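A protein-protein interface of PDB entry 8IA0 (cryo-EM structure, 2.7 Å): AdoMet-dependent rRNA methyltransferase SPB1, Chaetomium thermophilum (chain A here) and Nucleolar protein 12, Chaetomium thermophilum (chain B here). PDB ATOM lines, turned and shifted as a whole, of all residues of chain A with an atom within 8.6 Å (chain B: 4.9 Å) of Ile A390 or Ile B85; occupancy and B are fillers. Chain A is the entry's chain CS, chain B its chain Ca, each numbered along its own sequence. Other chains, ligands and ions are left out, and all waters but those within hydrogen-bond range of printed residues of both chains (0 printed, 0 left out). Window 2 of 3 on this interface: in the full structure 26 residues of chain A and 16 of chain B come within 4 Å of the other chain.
The side-chain amide nitrogen (NE2) of Gln A394 lies within hydrogen-bond range of a ring nitrogen (ND1) of His B81.
The backbone carbonyl oxygen (O) of Gln A394 sits at hydrogen-bond distance from the side-chain hydroxyl (OG1) of Thr A398 (2.4 Å). The side-chain hydroxyl (OG1) of Thr A398 sits at hydrogen-bond distance from the backbone carbonyl oxygen (O) of Met A395. O of Ile B82 lies close to OD1 of Asn B86 (2.9 Å).
CG2 of Ile A390 touches CD1 of Ile B82, at 3.6 Å. CG2 of Ile B85 touches CG2 of Ile A390, 3.6 Å away. Ile A390 touches Asn B86. CG of His B81 touches CE of Met A397 (3.5 Å). His B81 touches Thr A398.
Of the printed residues of chain B, Gln A394 touches His B81. Of the printed residues of chain B, Met A397 touches His B81 (3.5 Å). Of the printed residues of chain B, Thr A398 touches His B81. No residue of chain A comes within 4 Å of Ala B84. Of the printed residues of chain A, Ile B85 touches Ile A390. Asn B86 touches one residue of chain A. Leu B89 touches none of the printed residues of chain A. The nearest residue of chain A that does not touch Ile B85 is Met A397 (4.2 Å). The nearest printed residue of chain A that does not touch Ile B82 is Val A391 (4.2 Å).
Of the 16 printed residues of chain A, 4 touch a printed residue of chain B. Hydrophobic or aromatic side chains of chain A that line the printed part of chain B: Ile A390 and Met A397. Among the printed residues, no Asp or Glu carboxylate lies within 4 Å of a Lys or Arg side-chain nitrogen of the other chain.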
ATOM      1  N   ASN A 383      -9.281  26.475  18.446  1.00  0.00           N
ATOM      2  CA  ASN A 383      -9.288  27.454  17.365  1.00  0.00           C
ATOM      3  C   ASN A 383      -8.323  27.057  16.256  1.00  0.00           C
ATOM      4  O   ASN A 383      -8.645  27.170  15.068  1.00  0.00           O
ATOM      5  CB  ASN A 383      -8.938  28.838  17.914  1.00  0.00           C
ATOM      6  CG  ASN A 383      -9.690  29.949  17.211  1.00  0.00           C
ATOM      7  OD1 ASN A 383      -9.608  30.096  15.992  1.00  0.00           O
ATOM      8  ND2 ASN A 383     -10.431  30.740  17.979  1.00  0.00           N
ATOM      9  N   GLU A 384      -7.130  26.586  16.624  1.00  0.00           N
ATOM     10  CA  GLU A 384      -6.122  26.270  15.616  1.00  0.00           C
ATOM     11  C   GLU A 384      -6.439  24.964  14.897  1.00  0.00           C
ATOM     12  O   GLU A 384      -6.114  24.810  13.714  1.00  0.00           O
ATOM     13  CB  GLU A 384      -4.732  26.224  16.254  1.00  0.00           C
ATOM     14  CG  GLU A 384      -4.495  25.053  17.194  1.00  0.00           C
ATOM     15  CD  GLU A 384      -3.125  25.095  17.844  1.00  0.00           C
ATOM     16  OE1 GLU A 384      -2.369  26.053  17.581  1.00  0.00           O
ATOM     17  OE2 GLU A 384      -2.805  24.169  18.619  1.00  0.00           O
ATOM     18  N   ARG A 385      -7.061  24.006  15.591  1.00  0.00           N
ATOM     19  CA  ARG A 385      -7.454  22.763  14.932  1.00  0.00           C
ATOM     20  C   ARG A 385      -8.506  23.019  13.862  1.00  0.00           C
ATOM     21  O   ARG A 385      -8.434  22.455  12.763  1.00  0.00           O
ATOM     22  CB  ARG A 385      -7.969  21.755  15.957  1.00  0.00           C
ATOM     23  CG  ARG A 385      -6.887  21.158  16.836  1.00  0.00           C
ATOM     24  CD  ARG A 385      -7.469  20.147  17.808  1.00  0.00           C
ATOM     25  NE  ARG A 385      -8.038  18.997  17.116  1.00  0.00           N
ATOM     26  CZ  ARG A 385      -7.357  17.911  16.782  1.00  0.00           C
ATOM     27  NH1 ARG A 385      -6.069  17.788  17.061  1.00  0.00           N
ATOM     28  NH2 ARG A 385      -7.983  16.922  16.149  1.00  0.00           N
ATOM     29  N   LYS A 386      -9.497  23.858  14.168  1.00  0.00           N
ATOM     30  CA  LYS A 386     -10.481  24.234  13.161  1.00  0.00           C
ATOM     31  C   LYS A 386      -9.827  25.004  12.023  1.00  0.00           C
ATOM     32  O   LYS A 386     -10.164  24.804  10.850  1.00  0.00           O
ATOM     33  CB  LYS A 386     -11.595  25.060  13.804  1.00  0.00           C
ATOM     34  CG  LYS A 386     -12.632  25.582  12.825  1.00  0.00           C
ATOM     35  CD  LYS A 386     -13.851  26.123  13.552  1.00  0.00           C
ATOM     36  CE  LYS A 386     -15.055  25.215  13.368  1.00  0.00           C
ATOM     37  NZ  LYS A 386     -14.665  23.781  13.261  1.00  0.00           N
ATOM     38  N   HIS A 387      -8.884  25.888  12.352  1.00  0.00           N
ATOM     39  CA  HIS A 387      -8.178  26.643  11.323  1.00  0.00           C
ATOM     40  C   HIS A 387      -7.390  25.714  10.411  1.00  0.00           C
ATOM     41  O   HIS A 387      -7.332  25.928   9.195  1.00  0.00           O
ATOM     42  CB  HIS A 387      -7.262  27.676  11.983  1.00  0.00           C
ATOM     43  CG  HIS A 387      -6.608  28.624  11.025  1.00  0.00           C
ATOM     44  ND1 HIS A 387      -5.975  28.213   9.872  1.00  0.00           N
ATOM     45  CD2 HIS A 387      -6.489  29.972  11.055  1.00  0.00           C
ATOM     46  CE1 HIS A 387      -5.495  29.265   9.234  1.00  0.00           C
ATOM     47  NE2 HIS A 387      -5.795  30.345   9.931  1.00  0.00           N
ATOM     48  N   LYS A 388      -6.767  24.680  10.981  1.00  0.00           N
ATOM     49  CA  LYS A 388      -5.987  23.750  10.171  1.00  0.00           C
ATOM     50  C   LYS A 388      -6.874  23.001   9.185  1.00  0.00           C
ATOM     51  O   LYS A 388      -6.472  22.750   8.043  1.00  0.00           O
ATOM     52  CB  LYS A 388      -5.234  22.774  11.074  1.00  0.00           C
ATOM     53  CG  LYS A 388      -3.783  22.567  10.678  1.00  0.00           C
ATOM     54  CD  LYS A 388      -3.051  21.700  11.687  1.00  0.00           C
ATOM     55  CE  LYS A 388      -1.660  21.336  11.195  1.00  0.00           C
ATOM     56  NZ  LYS A 388      -1.633  21.091   9.727  1.00  0.00           N
ATOM     57  N   GLU A 389      -8.085  22.632   9.608  1.00  0.00           N
ATOM     58  CA  GLU A 389      -9.017  21.967   8.702  1.00  0.00           C
ATOM     59  C   GLU A 389      -9.445  22.883   7.564  1.00  0.00           C
ATOM     60  O   GLU A 389      -9.515  22.451   6.409  1.00  0.00           O
ATOM     61  CB  GLU A 389     -10.240  21.475   9.472  1.00  0.00           C
ATOM     62  CG  GLU A 389      -9.976  20.301  10.393  1.00  0.00           C
ATOM     63  CD  GLU A 389      -9.999  18.971   9.662  1.00  0.00           C
ATOM     64  OE1 GLU A 389     -10.393  17.966  10.284  1.00  0.00           O
ATOM     65  OE2 GLU A 389      -9.624  18.922   8.471  1.00  0.00           O
ATOM     66  N   ILE A 390      -9.739  24.146   7.872  1.00  0.00           N
ATOM     67  CA  ILE A 390     -10.196  25.077   6.843  1.00  0.00           C
ATOM     68  C   ILE A 390      -9.128  25.249   5.771  1.00  0.00           C
ATOM     69  O   ILE A 390      -9.436  25.359   4.578  1.00  0.00           O
ATOM     70  CB  ILE A 390     -10.592  26.420   7.483  1.00  0.00           C
ATOM     71  CG1 ILE A 390     -11.856  26.248   8.325  1.00  0.00           C
ATOM     72  CG2 ILE A 390     -10.810  27.482   6.424  1.00  0.00           C
ATOM     73  CD1 ILE A 390     -12.202  27.457   9.162  1.00  0.00           C
ATOM     74  N   VAL A 391      -7.859  25.263   6.177  1.00  0.00           N
ATOM     75  CA  VAL A 391      -6.767  25.329   5.211  1.00  0.00           C
ATOM     76  C   VAL A 391      -6.759  24.086   4.330  1.00  0.00           C
ATOM     77  O   VAL A 391      -6.475  24.160   3.129  1.00  0.00           O
ATOM     78  CB  VAL A 391      -5.425  25.519   5.944  1.00  0.00           C
ATOM     79  CG1 VAL A 391      -4.258  25.371   4.982  1.00  0.00           C
ATOM     80  CG2 VAL A 391      -5.389  26.872   6.634  1.00  0.00           C
ATOM     81  N   ARG A 392      -7.076  22.925   4.912  1.00  0.00           N
ATOM     82  CA  ARG A 392      -7.072  21.684   4.142  1.00  0.00           C
ATOM     83  C   ARG A 392      -8.109  21.714   3.027  1.00  0.00           C
ATOM     84  O   ARG A 392      -7.819  21.318   1.892  1.00  0.00           O
ATOM     85  CB  ARG A 392      -7.315  20.493   5.066  1.00  0.00           C
ATOM     86  CG  ARG A 392      -6.046  19.893   5.636  1.00  0.00           C
ATOM     87  CD  ARG A 392      -5.989  18.401   5.383  1.00  0.00           C
ATOM     88  NE  ARG A 392      -7.094  17.701   6.025  1.00  0.00           N
ATOM     89  CZ  ARG A 392      -7.277  16.390   5.974  1.00  0.00           C
ATOM     90  NH1 ARG A 392      -6.447  15.602   5.311  1.00  0.00           N
ATOM     91  NH2 ARG A 392      -8.318  15.856   6.605  1.00  0.00           N
ATOM     92  N   MET A 393      -9.325  22.174   3.328  1.00  0.00           N
ATOM     93  CA  MET A 393     -10.332  22.317   2.281  1.00  0.00           C
ATOM     94  C   MET A 393      -9.938  23.398   1.287  1.00  0.00           C
ATOM     95  O   MET A 393     -10.203  23.276   0.086  1.00  0.00           O
ATOM     96  CB  MET A 393     -11.697  22.626   2.893  1.00  0.00           C
ATOM     97  CG  MET A 393     -12.443  21.404   3.388  1.00  0.00           C
ATOM     98  SD  MET A 393     -11.913  20.912   5.036  1.00  0.00           S
ATOM     99  CE  MET A 393     -12.712  22.177   6.017  1.00  0.00           C
ATOM    100  N   GLN A 394      -9.310  24.471   1.771  1.00  0.00           N
ATOM    101  CA  GLN A 394      -8.843  25.523   0.876  1.00  0.00           C
ATOM    102  C   GLN A 394      -7.800  24.988  -0.097  1.00  0.00           C
ATOM    103  O   GLN A 394      -7.826  25.308  -1.291  1.00  0.00           O
ATOM    104  CB  GLN A 394      -8.276  26.685   1.690  1.00  0.00           C
ATOM    105  CG  GLN A 394      -8.084  27.959   0.891  1.00  0.00           C
ATOM    106  CD  GLN A 394      -6.729  28.027   0.221  1.00  0.00           C
ATOM    107  OE1 GLN A 394      -5.771  27.395   0.665  1.00  0.00           O
ATOM    108  NE2 GLN A 394      -6.641  28.798  -0.857  1.00  0.00           N
ATOM    109  N   MET A 395      -6.868  24.172   0.398  1.00  0.00           N
ATOM    110  CA  MET A 395      -5.866  23.581  -0.482  1.00  0.00           C
ATOM    111  C   MET A 395      -6.511  22.626  -1.478  1.00  0.00           C
ATOM    112  O   MET A 395      -6.096  22.556  -2.641  1.00  0.00           O
ATOM    113  CB  MET A 395      -4.796  22.865   0.346  1.00  0.00           C
ATOM    114  CG  MET A 395      -4.224  21.612  -0.305  1.00  0.00           C
ATOM    115  SD  MET A 395      -3.153  20.654   0.788  1.00  0.00           S
ATOM    116  CE  MET A 395      -4.136  20.609   2.283  1.00  0.00           C
ATOM    117  N   HIS A 396      -7.533  21.888  -1.040  1.00  0.00           N
ATOM    118  CA  HIS A 396      -8.202  20.942  -1.926  1.00  0.00           C
ATOM    119  C   HIS A 396      -8.874  21.652  -3.094  1.00  0.00           C
ATOM    120  O   HIS A 396      -8.828  21.171  -4.232  1.00  0.00           O
ATOM    121  CB  HIS A 396      -9.221  20.119  -1.139  1.00  0.00           C
ATOM    122  CG  HIS A 396      -8.612  19.042  -0.298  1.00  0.00           C
ATOM    123  ND1 HIS A 396      -7.544  18.280  -0.722  1.00  0.00           N
ATOM    124  CD2 HIS A 396      -8.921  18.599   0.944  1.00  0.00           C
ATOM    125  CE1 HIS A 396      -7.222  17.414   0.223  1.00  0.00           C
ATOM    126  NE2 HIS A 396      -8.042  17.586   1.244  1.00  0.00           N
ATOM    127  N   MET A 397      -9.505  22.798  -2.835  1.00  0.00           N
ATOM    128  CA  MET A 397     -10.191  23.533  -3.889  1.00  0.00           C
ATOM    129  C   MET A 397      -9.270  24.463  -4.666  1.00  0.00           C
ATOM    130  O   MET A 397      -9.729  25.116  -5.609  1.00  0.00           O
ATOM    131  CB  MET A 397     -11.359  24.334  -3.304  1.00  0.00           C
ATOM    132  CG  MET A 397     -10.986  25.691  -2.730  1.00  0.00           C
ATOM    133  SD  MET A 397     -12.305  26.365  -1.700  1.00  0.00           S
ATOM    134  CE  MET A 397     -11.408  27.569  -0.726  1.00  0.00           C
ATOM    135  N   THR A 398      -7.993  24.538  -4.305  1.00  0.00           N
ATOM    136  CA  THR A 398      -7.042  25.371  -5.031  1.00  0.00           C
ATOM    137  C   THR A 398      -5.941  24.520  -5.655  1.00  0.00           C
ATOM    138  O   THR A 398      -6.214  23.617  -6.447  1.00  0.00           O
ATOM    139  CB  THR A 398      -6.404  26.433  -4.118  1.00  0.00           C
ATOM    140  OG1 THR A 398      -6.030  25.835  -2.871  1.00  0.00           O
ATOM    141  CG2 THR A 398      -7.383  27.568  -3.860  1.00  0.00           C
ATOM    142  N   HIS B  81     -10.270  33.235   1.122  1.00  0.00           N
ATOM    143  CA  HIS B  81     -10.941  31.939   1.132  1.00  0.00           C
ATOM    144  C   HIS B  81     -11.273  31.501   2.552  1.00  0.00           C
ATOM    145  O   HIS B  81     -12.344  30.933   2.800  1.00  0.00           O
ATOM    146  CB  HIS B  81     -10.074  30.891   0.436  1.00  0.00           C
ATOM    147  CG  HIS B  81     -10.205  30.888  -1.055  1.00  0.00           C
ATOM    148  ND1 HIS B  81      -9.299  30.257  -1.880  1.00  0.00           N
ATOM    149  CD2 HIS B  81     -11.141  31.431  -1.869  1.00  0.00           C
ATOM    150  CE1 HIS B  81      -9.668  30.416  -3.138  1.00  0.00           C
ATOM    151  NE2 HIS B  81     -10.782  31.125  -3.160  1.00  0.00           N
ATOM    152  N   ILE B  82     -10.364  31.748   3.497  1.00  0.00           N
ATOM    153  CA  ILE B  82     -10.600  31.352   4.882  1.00  0.00           C
ATOM    154  C   ILE B  82     -11.791  32.108   5.456  1.00  0.00           C
ATOM    155  O   ILE B  82     -12.644  31.526   6.138  1.00  0.00           O
ATOM    156  CB  ILE B  82      -9.330  31.576   5.724  1.00  0.00           C
ATOM    157  CG1 ILE B  82      -8.112  30.960   5.033  1.00  0.00           C
ATOM    158  CG2 ILE B  82      -9.507  30.994   7.119  1.00  0.00           C
ATOM    159  CD1 ILE B  82      -8.192  29.460   4.865  1.00  0.00           C
ATOM    160  N   LYS B  83     -11.866  33.414   5.194  1.00  0.00           N
ATOM    161  CA  LYS B  83     -12.975  34.212   5.708  1.00  0.00           C
ATOM    162  C   LYS B  83     -14.301  33.781   5.095  1.00  0.00           C
ATOM    163  O   LYS B  83     -15.324  33.734   5.789  1.00  0.00           O
ATOM    164  CB  LYS B  83     -12.719  35.696   5.451  1.00  0.00           C
ATOM    165  CG  LYS B  83     -12.339  36.481   6.697  1.00  0.00           C
ATOM    166  CD  LYS B  83     -10.951  36.106   7.189  1.00  0.00           C
ATOM    167  CE  LYS B  83      -9.871  36.722   6.316  1.00  0.00           C
ATOM    168  NZ  LYS B  83      -8.504  36.404   6.817  1.00  0.00           N
ATOM    169  N   ALA B  84     -14.306  33.473   3.797  1.00  0.00           N
ATOM    170  CA  ALA B  84     -15.536  33.027   3.149  1.00  0.00           C
ATOM    171  C   ALA B  84     -16.036  31.723   3.756  1.00  0.00           C
ATOM    172  O   ALA B  84     -17.240  31.561   3.991  1.00  0.00           O
ATOM    173  CB  ALA B  84     -15.312  32.871   1.646  1.00  0.00           C
ATOM    174  N   ILE B  85     -15.128  30.780   4.012  1.00  0.00           N
ATOM    175  CA  ILE B  85     -15.519  29.534   4.665  1.00  0.00           C
ATOM    176  C   ILE B  85     -15.953  29.803   6.100  1.00  0.00           C
ATOM    177  O   ILE B  85     -16.948  29.245   6.579  1.00  0.00           O
ATOM    178  CB  ILE B  85     -14.370  28.510   4.594  1.00  0.00           C
ATOM    179  CG1 ILE B  85     -14.481  27.677   3.316  1.00  0.00           C
ATOM    180  CG2 ILE B  85     -14.382  27.595   5.810  1.00  0.00           C
ATOM    181  CD1 ILE B  85     -13.231  26.887   2.993  1.00  0.00           C
ATOM    182  N   ASN B  86     -15.216  30.663   6.807  1.00  0.00           N
ATOM    183  CA  ASN B  86     -15.598  31.011   8.172  1.00  0.00           C
ATOM    184  C   ASN B  86     -16.963  31.684   8.203  1.00  0.00           C
ATOM    185  O   ASN B  86     -17.780  31.406   9.089  1.00  0.00           O
ATOM    186  CB  ASN B  86     -14.539  31.915   8.801  1.00  0.00           C
ATOM    187  CG  ASN B  86     -13.430  31.131   9.475  1.00  0.00           C
ATOM    188  OD1 ASN B  86     -12.290  31.120   9.010  1.00  0.00           O
ATOM    189  ND2 ASN B  86     -13.759  30.469  10.579  1.00  0.00           N
ATOM    190  N   LYS B  87     -17.225  32.577   7.248  1.00  0.00           N
ATOM    191  CA  LYS B  87     -18.549  33.183   7.146  1.00  0.00           C
ATOM    192  C   LYS B  87     -19.604  32.131   6.831  1.00  0.00           C
ATOM    193  O   LYS B  87     -20.672  32.102   7.452  1.00  0.00           O
ATOM    194  CB  LYS B  87     -18.535  34.290   6.085  1.00  0.00           C
ATOM    195  CG  LYS B  87     -19.891  34.643   5.470  1.00  0.00           C
ATOM    196  CD  LYS B  87     -20.162  33.892   4.167  1.00  0.00           C
ATOM    197  CE  LYS B  87     -19.150  34.253   3.091  1.00  0.00           C
ATOM    198  NZ  LYS B  87     -19.203  33.304   1.944  1.00  0.00           N
ATOM    199  N   ILE B  88     -19.311  31.246   5.873  1.00  0.00           N
ATOM    200  CA  ILE B  88     -20.290  30.247   5.455  1.00  0.00           C
ATOM    201  C   ILE B  88     -20.519  29.216   6.550  1.00  0.00           C
ATOM    202  O   ILE B  88     -21.546  28.526   6.561  1.00  0.00           O
ATOM    203  CB  ILE B  88     -19.851  29.589   4.130  1.00  0.00           C
ATOM    204  CG1 ILE B  88     -21.069  29.276   3.261  1.00  0.00           C
ATOM    205  CG2 ILE B  88     -19.043  28.336   4.391  1.00  0.00           C
ATOM    206  CD1 ILE B  88     -21.794  30.506   2.761  1.00  0.00           C
ATOM    207  N   LEU B  89     -19.576  29.088   7.484  1.00  0.00           N
ATOM    208  CA  LEU B  89     -19.792  28.208   8.626  1.00  0.00           C
ATOM    209  C   LEU B  89     -20.658  28.883   9.683  1.00  0.00           C
ATOM    210  O   LEU B  89     -21.274  28.205  10.513  1.00  0.00           O
ATOM    211  CB  LEU B  89     -18.450  27.782   9.223  1.00  0.00           C
ATOM    212  CG  LEU B  89     -17.840  26.483   8.692  1.00  0.00           C
ATOM    213  CD1 LEU B  89     -16.374  26.381   9.080  1.00  0.00           C
ATOM    214  CD2 LEU B  89     -18.618  25.280   9.199  1.00  0.00           C
